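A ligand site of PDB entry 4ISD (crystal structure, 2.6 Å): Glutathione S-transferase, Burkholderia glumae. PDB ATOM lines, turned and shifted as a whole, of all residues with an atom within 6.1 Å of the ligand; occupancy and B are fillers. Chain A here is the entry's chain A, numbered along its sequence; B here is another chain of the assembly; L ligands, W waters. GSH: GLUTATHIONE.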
ATOM      1  N   SER A  18      10.791  -8.880  13.030  1.00  0.00           N
ATOM      2  CA  SER A  18      10.639  -8.162  11.758  1.00  0.00           C
ATOM      3  C   SER A  18       9.918  -6.808  11.826  1.00  0.00           C
ATOM      4  O   SER A  18       8.800  -6.703  12.324  1.00  0.00           O
ATOM      5  CB  SER A  18       9.927  -9.042  10.725  1.00  0.00           C
ATOM      6  OG  SER A  18       9.671  -8.315   9.533  1.00  0.00           O
ATOM      7  N   ALA A  19      10.561  -5.774  11.297  1.00  0.00           N
ATOM      8  CA  ALA A  19       9.949  -4.458  11.198  1.00  0.00           C
ATOM      9  C   ALA A  19       8.816  -4.480  10.187  1.00  0.00           C
ATOM     10  O   ALA A  19       7.935  -3.607  10.179  1.00  0.00           O
ATOM     11  CB  ALA A  19      10.971  -3.451  10.759  1.00  0.00           C
ATOM     12  N   PHE A  20       8.836  -5.467   9.305  1.00  0.00           N
ATOM     13  CA  PHE A  20       7.898  -5.502   8.200  1.00  0.00           C
ATOM     14  C   PHE A  20       6.680  -6.338   8.547  1.00  0.00           C
ATOM     15  O   PHE A  20       5.578  -6.044   8.085  1.00  0.00           O
ATOM     16  CB  PHE A  20       8.598  -6.017   6.937  1.00  0.00           C
ATOM     17  CG  PHE A  20       9.798  -5.189   6.558  1.00  0.00           C
ATOM     18  CD1 PHE A  20       9.651  -3.833   6.305  1.00  0.00           C
ATOM     19  CD2 PHE A  20      11.057  -5.765   6.476  1.00  0.00           C
ATOM     20  CE1 PHE A  20      10.762  -3.051   5.971  1.00  0.00           C
ATOM     21  CE2 PHE A  20      12.169  -5.006   6.143  1.00  0.00           C
ATOM     22  CZ  PHE A  20      12.021  -3.640   5.886  1.00  0.00           C
ATOM     23  N   GLN A  46      11.161 -20.931   6.347  1.00  0.00           N
ATOM     24  CA  GLN A  46      10.645 -20.226   5.173  1.00  0.00           C
ATOM     25  C   GLN A  46      10.978 -20.966   3.865  1.00  0.00           C
ATOM     26  O   GLN A  46      10.800 -20.440   2.762  1.00  0.00           O
ATOM     27  CB  GLN A  46      11.146 -18.766   5.115  1.00  0.00           C
ATOM     28  CG  GLN A  46      12.651 -18.611   4.841  1.00  0.00           C
ATOM     29  CD  GLN A  46      13.483 -18.599   6.127  1.00  0.00           C
ATOM     30  OE1 GLN A  46      13.129 -19.224   7.134  1.00  0.00           O
ATOM     31  NE2 GLN A  46      14.595 -17.859   6.096  1.00  0.00           N
ATOM     32  N   GLN A  47      11.464 -22.205   4.003  1.00  0.00           N
ATOM     33  CA  GLN A  47      11.815 -23.019   2.845  1.00  0.00           C
ATOM     34  C   GLN A  47      11.411 -24.497   3.025  1.00  0.00           C
ATOM     35  O   GLN A  47      10.221 -24.840   3.200  1.00  0.00           O
ATOM     36  CB  GLN A  47      13.320 -22.855   2.565  1.00  0.00           C
ATOM     37  CG  GLN A  47      13.654 -21.542   1.838  1.00  0.00           C
ATOM     38  CD  GLN A  47      14.647 -20.640   2.576  1.00  0.00           C
ATOM     39  OE1 GLN A  47      15.105 -20.969   3.664  1.00  0.00           O
ATOM     40  NE2 GLN A  47      14.966 -19.490   1.967  1.00  0.00           N
ATOM     41  N   THR A  58       7.817 -15.332  -2.281  1.00  0.00           N
ATOM     42  CA  THR A  58       9.115 -14.746  -1.975  1.00  0.00           C
ATOM     43  C   THR A  58       9.885 -15.469  -0.865  1.00  0.00           C
ATOM     44  O   THR A  58      11.089 -15.243  -0.690  1.00  0.00           O
ATOM     45  CB  THR A  58       8.945 -13.303  -1.512  1.00  0.00           C
ATOM     46  OG1 THR A  58       8.284 -13.292  -0.240  1.00  0.00           O
ATOM     47  CG2 THR A  58       8.108 -12.539  -2.512  1.00  0.00           C
ATOM     48  N   ARG A  59       9.182 -16.301  -0.110  1.00  0.00           N
ATOM     49  CA  ARG A  59       9.737 -16.982   1.064  1.00  0.00           C
ATOM     50  C   ARG A  59      10.273 -16.007   2.110  1.00  0.00           C
ATOM     51  O   ARG A  59      11.325 -16.230   2.713  1.00  0.00           O
ATOM     52  CB  ARG A  59      10.831 -17.976   0.659  1.00  0.00           C
ATOM     53  CG  ARG A  59      10.368 -19.041  -0.328  1.00  0.00           C
ATOM     54  CD  ARG A  59      11.425 -20.114  -0.433  1.00  0.00           C
ATOM     55  NE  ARG A  59      11.758 -20.447  -1.818  1.00  0.00           N
ATOM     56  CZ  ARG A  59      12.852 -21.100  -2.180  1.00  0.00           C
ATOM     57  NH1 ARG A  59      13.749 -21.466  -1.259  1.00  0.00           N
ATOM     58  NH2 ARG A  59      13.077 -21.373  -3.457  1.00  0.00           N
ATOM     59  N   ARG A  60       9.552 -14.919   2.300  1.00  0.00           N
ATOM     60  CA  ARG A  60       9.839 -14.008   3.389  1.00  0.00           C
ATOM     61  C   ARG A  60       8.549 -13.694   4.169  1.00  0.00           C
ATOM     62  O   ARG A  60       7.433 -13.815   3.637  1.00  0.00           O
ATOM     63  CB  ARG A  60      10.489 -12.731   2.857  1.00  0.00           C
ATOM     64  CG  ARG A  60      11.758 -13.007   2.064  1.00  0.00           C
ATOM     65  CD  ARG A  60      12.604 -11.750   1.918  1.00  0.00           C
ATOM     66  NE  ARG A  60      11.902 -10.715   1.175  1.00  0.00           N
ATOM     67  CZ  ARG A  60      12.485  -9.580   0.780  1.00  0.00           C
ATOM     68  NH1 ARG A  60      11.788  -8.675   0.091  1.00  0.00           N
ATOM     69  NH2 ARG A  60      13.765  -9.378   1.067  1.00  0.00           N
ATOM     70  N   VAL A  61       8.700 -13.335   5.434  1.00  0.00           N
ATOM     71  CA  VAL A  61       7.580 -12.859   6.224  1.00  0.00           C
ATOM     72  C   VAL A  61       7.618 -11.341   6.134  1.00  0.00           C
ATOM     73  O   VAL A  61       8.693 -10.758   5.995  1.00  0.00           O
ATOM     74  CB  VAL A  61       7.670 -13.323   7.691  1.00  0.00           C
ATOM     75  CG1 VAL A  61       7.420 -14.819   7.811  1.00  0.00           C
ATOM     76  CG2 VAL A  61       9.030 -12.960   8.285  1.00  0.00           C
ATOM     77  N   PRO A  62       6.445 -10.681   6.196  1.00  0.00           N
ATOM     78  CA  PRO A  62       5.078 -11.218   6.309  1.00  0.00           C
ATOM     79  C   PRO A  62       4.487 -11.748   4.997  1.00  0.00           C
ATOM     80  O   PRO A  62       4.911 -11.401   3.892  1.00  0.00           O
ATOM     81  CB  PRO A  62       4.290  -9.982   6.733  1.00  0.00           C
ATOM     82  CG  PRO A  62       4.997  -8.875   5.991  1.00  0.00           C
ATOM     83  CD  PRO A  62       6.442  -9.209   6.188  1.00  0.00           C
ATOM     84  N   SER A  72       2.503 -11.659  -0.351  1.00  0.00           N
ATOM     85  CA  SER A  72       3.682 -11.239   0.428  1.00  0.00           C
ATOM     86  C   SER A  72       4.058  -9.772   0.194  1.00  0.00           C
ATOM     87  O   SER A  72       3.334  -9.058  -0.523  1.00  0.00           O
ATOM     88  CB  SER A  72       4.877 -12.159   0.161  1.00  0.00           C
ATOM     89  OG  SER A  72       4.803 -13.341   0.957  1.00  0.00           O
ATOM     90  N   GLU A  73       5.163  -9.320   0.775  1.00  0.00           N
ATOM     91  CA  GLU A  73       5.597  -7.905   0.704  1.00  0.00           C
ATOM     92  C   GLU A  73       4.614  -6.978   1.424  1.00  0.00           C
ATOM     93  O   GLU A  73       3.515  -6.684   0.904  1.00  0.00           O
ATOM     94  CB  GLU A  73       5.836  -7.434  -0.732  1.00  0.00           C
ATOM     95  CG  GLU A  73       6.957  -8.158  -1.469  1.00  0.00           C
ATOM     96  CD  GLU A  73       8.320  -7.848  -0.867  1.00  0.00           C
ATOM     97  OE1 GLU A  73       8.617  -6.642  -0.732  1.00  0.00           O
ATOM     98  OE2 GLU A  73       9.073  -8.798  -0.531  1.00  0.00           O
ATOM     99  N   SER A  74       5.043  -6.502   2.594  1.00  0.00           N
ATOM    100  CA  SER A  74       4.213  -5.740   3.515  1.00  0.00           C
ATOM    101  C   SER A  74       3.603  -4.473   2.921  1.00  0.00           C
ATOM    102  O   SER A  74       2.440  -4.146   3.226  1.00  0.00           O
ATOM    103  CB  SER A  74       5.006  -5.391   4.785  1.00  0.00           C
ATOM    104  OG  SER A  74       5.994  -4.426   4.531  1.00  0.00           O
ATOM    105  N   SER A  75       4.347  -3.775   2.074  1.00  0.00           N
ATOM    106  CA  SER A  75       3.785  -2.601   1.399  1.00  0.00           C
ATOM    107  C   SER A  75       2.632  -3.009   0.463  1.00  0.00           C
ATOM    108  O   SER A  75       1.583  -2.366   0.451  1.00  0.00           O
ATOM    109  CB  SER A  75       4.859  -1.779   0.666  1.00  0.00           C
ATOM    110  OG  SER A  75       5.321  -2.400  -0.528  1.00  0.00           O
ATOM    111  N   ARG A 112      12.374   0.222   2.492  1.00  0.00           N
ATOM    112  CA  ARG A 112      12.525  -1.180   2.178  1.00  0.00           C
ATOM    113  C   ARG A 112      13.683  -1.500   1.218  1.00  0.00           C
ATOM    114  O   ARG A 112      14.007  -2.677   1.039  1.00  0.00           O
ATOM    115  CB  ARG A 112      11.224  -1.701   1.589  1.00  0.00           C
ATOM    116  CG  ARG A 112      10.102  -1.860   2.603  1.00  0.00           C
ATOM    117  CD  ARG A 112       8.753  -2.021   1.938  1.00  0.00           C
ATOM    118  NE  ARG A 112       7.718  -2.284   2.926  1.00  0.00           N
ATOM    119  CZ  ARG A 112       7.223  -1.379   3.776  1.00  0.00           C
ATOM    120  NH1 ARG A 112       7.684  -0.121   3.753  1.00  0.00           N
ATOM    121  NH2 ARG A 112       6.287  -1.731   4.649  1.00  0.00           N
ATOM    122  N   ALA B 109       7.936  -4.820  -5.508  1.00  0.00           N
ATOM    123  CA  ALA B 109       8.607  -4.626  -4.237  1.00  0.00           C
ATOM    124  C   ALA B 109       9.602  -5.758  -3.928  1.00  0.00           C
ATOM    125  O   ALA B 109      10.647  -5.530  -3.289  1.00  0.00           O
ATOM    126  CB  ALA B 109       7.601  -4.450  -3.098  1.00  0.00           C
ATOM    127  N   TRP B 110       9.287  -6.965  -4.378  1.00  0.00           N
ATOM    128  CA  TRP B 110      10.204  -8.089  -4.149  1.00  0.00           C
ATOM    129  C   TRP B 110      11.499  -7.811  -4.872  1.00  0.00           C
ATOM    130  O   TRP B 110      12.591  -7.853  -4.280  1.00  0.00           O
ATOM    131  CB  TRP B 110       9.605  -9.395  -4.631  1.00  0.00           C
ATOM    132  CG  TRP B 110      10.402 -10.606  -4.267  1.00  0.00           C
ATOM    133  CD1 TRP B 110      11.260 -10.740  -3.207  1.00  0.00           C
ATOM    134  CD2 TRP B 110      10.409 -11.863  -4.956  1.00  0.00           C
ATOM    135  NE1 TRP B 110      11.803 -12.007  -3.200  1.00  0.00           N
ATOM    136  CE2 TRP B 110      11.293 -12.713  -4.263  1.00  0.00           C
ATOM    137  CE3 TRP B 110       9.738 -12.352  -6.076  1.00  0.00           C
ATOM    138  CZ2 TRP B 110      11.533 -14.026  -4.668  1.00  0.00           C
ATOM    139  CZ3 TRP B 110       9.988 -13.656  -6.487  1.00  0.00           C
ATOM    140  CH2 TRP B 110      10.880 -14.473  -5.778  1.00  0.00           C
ATOM    141  N   SER B 113      13.869  -5.215  -3.336  1.00  0.00           N
ATOM    142  CA  SER B 113      14.326  -5.384  -1.959  1.00  0.00           C
ATOM    143  C   SER B 113      14.806  -6.805  -1.656  1.00  0.00           C
ATOM    144  O   SER B 113      14.904  -7.192  -0.490  1.00  0.00           O
ATOM    145  CB  SER B 113      13.198  -5.053  -1.002  1.00  0.00           C
ATOM    146  OG  SER B 113      12.236  -6.108  -1.019  1.00  0.00           O
ATOM    147  N   ASP B 114      15.052  -7.606  -2.689  1.00  0.00           N
ATOM    148  CA  ASP B 114      15.648  -8.917  -2.443  1.00  0.00           C
ATOM    149  C   ASP B 114      16.727  -9.198  -3.491  1.00  0.00           C
ATOM    150  O   ASP B 114      17.113  -8.273  -4.207  1.00  0.00           O
ATOM    151  CB  ASP B 114      14.567 -10.004  -2.450  1.00  0.00           C
ATOM    152  CG  ASP B 114      14.988 -11.231  -1.660  1.00  0.00           C
ATOM    153  OD1 ASP B 114      16.183 -11.330  -1.307  1.00  0.00           O
ATOM    154  OD2 ASP B 114      14.125 -12.099  -1.408  1.00  0.00           O
ATOM    155  N   LEU B 142      20.966 -19.164  -3.087  1.00  0.00           N
ATOM    156  CA  LEU B 142      19.591 -19.118  -2.597  1.00  0.00           C
ATOM    157  C   LEU B 142      18.741 -18.110  -3.358  1.00  0.00           C
ATOM    158  O   LEU B 142      17.564 -18.364  -3.641  1.00  0.00           O
ATOM    159  CB  LEU B 142      19.576 -18.806  -1.107  1.00  0.00           C
ATOM    160  CG  LEU B 142      18.219 -18.847  -0.412  1.00  0.00           C
ATOM    161  CD1 LEU B 142      18.005 -20.176   0.321  1.00  0.00           C
ATOM    162  CD2 LEU B 142      18.054 -17.644   0.529  1.00  0.00           C
ATOM    163  N   LYS B 146      15.428 -18.856  -5.762  1.00  0.00           N
ATOM    164  CA  LYS B 146      14.130 -18.194  -5.571  1.00  0.00           C
ATOM    165  C   LYS B 146      13.700 -17.519  -6.861  1.00  0.00           C
ATOM    166  O   LYS B 146      12.525 -17.565  -7.244  1.00  0.00           O
ATOM    167  CB  LYS B 146      14.188 -17.166  -4.428  1.00  0.00           C
ATOM    168  CG  LYS B 146      14.190 -17.794  -3.034  1.00  0.00           C
ATOM    169  CD  LYS B 146      13.722 -16.812  -1.960  1.00  0.00           C
ATOM    170  CE  LYS B 146      14.631 -15.597  -1.844  1.00  0.00           C
ATOM    171  NZ  LYS B 146      14.096 -14.636  -0.820  1.00  0.00           N
HETATM  172  N1  GSH L   1      10.212  -5.789   1.381  1.00  0.00           N
HETATM  173  CA1 GSH L   1       9.811  -6.887   2.221  1.00  0.00           C
HETATM  174  C1  GSH L   1       8.506  -6.637   2.934  1.00  0.00           C
HETATM  175  O11 GSH L   1       8.128  -5.464   3.227  1.00  0.00           O
HETATM  176  O12 GSH L   1       7.790  -7.629   3.223  1.00  0.00           O
HETATM  177  CB1 GSH L   1      10.902  -7.335   3.169  1.00  0.00           C
HETATM  178  CG1 GSH L   1      10.447  -8.620   3.871  1.00  0.00           C
HETATM  179  CD1 GSH L   1      11.622  -9.203   4.684  1.00  0.00           C
HETATM  180  OE1 GSH L   1      12.755  -8.758   4.526  1.00  0.00           O
HETATM  181  N2  GSH L   1      11.386 -10.283   5.641  1.00  0.00           N
HETATM  182  CA2 GSH L   1      12.450 -10.861   6.431  1.00  0.00           C
HETATM  183  C2  GSH L   1      12.646 -12.299   6.072  1.00  0.00           C
HETATM  184  O2  GSH L   1      11.706 -12.994   5.740  1.00  0.00           O
HETATM  185  CB2 GSH L   1      12.120 -10.797   7.893  1.00  0.00           C
HETATM  186  SG2 GSH L   1      13.433  -9.960   8.739  1.00  0.00           S
HETATM  187  N3  GSH L   1      13.961 -12.895   6.111  1.00  0.00           N
HETATM  188  CA3 GSH L   1      14.075 -14.293   5.746  1.00  0.00           C
HETATM  189  C3  GSH L   1      14.810 -14.356   4.440  1.00  0.00           C
HETATM  190  O31 GSH L   1      14.831 -13.335   3.688  1.00  0.00           O
HETATM  191  O32 GSH L   1      15.424 -15.406   4.104  1.00  0.00           O
HETATM  192  O   HOH W   1       6.740 -10.283   2.631  1.00  0.00           O
HETATM  193  O   HOH W   2       6.871  -4.345   0.615  1.00  0.00           O
HETATM  194  O   HOH W   3      17.367 -17.311   3.564  1.00  0.00           O
HETATM  195  O   HOH W   4      14.079 -16.061   1.741  1.00  0.00           O
HETATM  196  O   HOH W   5      12.733  -4.914   2.302  1.00  0.00           O
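Water W4 lies within hydrogen-bond range of O32 of the ligand, O of Arg 59 and NZ of Lys 146 of chain B.
Water W5 bridges a nitrogen (N1) of the ligand (2.8 Å) and the backbone carbonyl oxygen (O) of Arg 112 (2.9 Å).
Water W1 lies within hydrogen-bond range of O of Pro 62 (2.5 Å), N of Glu 73 (2.6 Å) and O12 of the ligand (2.9 Å).
Water W2 lies within hydrogen-bond range of the side-chain hydroxyl (OG) of Ser 75, an oxygen (O11) of the ligand, the side-chain carboxylate (OE1) of Glu 73, the guanidinium group (NE) of Arg 112 and the backbone NH (N) of Ser 74.
Ser 18 touches the ligand (OG to CB2, 3.9 Å).
Phe 20 touches the ligand.
Arg 60 touches the ligand.
Pro 62 touches the ligand.
Of the 21 residues printed, 10 come within 4 Å of the ligand.
The side-chain hydroxyl of Ser 74 sits at hydrogen-bond distance from an oxygen (O11) of the ligand (2.7 Å).
The side-chain hydroxyl of Ser 113 of chain B sits at hydrogen-bond distance from a nitrogen (N1) of the ligand, at 3.2 Å.
The backbone NH (N) of Val 61 is in hydrogen-bond range of an oxygen (O2) of the ligand.
The backbone carbonyl oxygen (O) of Val 61 sits at hydrogen-bond distance from a nitrogen (N2) of the ligand.
The guanidinium group (NE) of Arg 112 is in salt-bridge range of an oxygen (O11) of the ligand, at 3.2 Å.
The side-chain amide nitrogen (NE2) of Gln 46 lies within hydrogen-bond range of an oxygen (O32) of the ligand (3.3 Å).
N1 of the ligand lies within salt-bridge range of OE1 of Glu 73 (2.8 Å).
N of Ser 74 is in hydrogen-bond range of O12 of the ligand, at 3.0 Å.
OG of Ser 18 lies within hydrogen-bond range of N of Phe 20 (3.0 Å).
The side-chain hydroxyl (OG) of Ser 74 sits at hydrogen-bond distance from the guanidinium group (NH2) of Arg 112 (2.7 Å).
OD2 of Asp 114 of chain B is in salt-bridge range of NE of Arg 60.
The backbone NH (N) of Arg 60 sits close to the side-chain hydroxyl (OG1) of Thr 58 (3.3 Å).
NH1 of Arg 60 is in hydrogen-bond range of OG of Ser 113 of chain B.
The side-chain hydroxyl of Ser 113 of chain B sits at hydrogen-bond distance from the backbone carbonyl oxygen of Ala 109 of chain B (2.8 Å).
OE2 of Glu 73 is in salt-bridge range of NH1 of Arg 60, at 2.8 Å.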
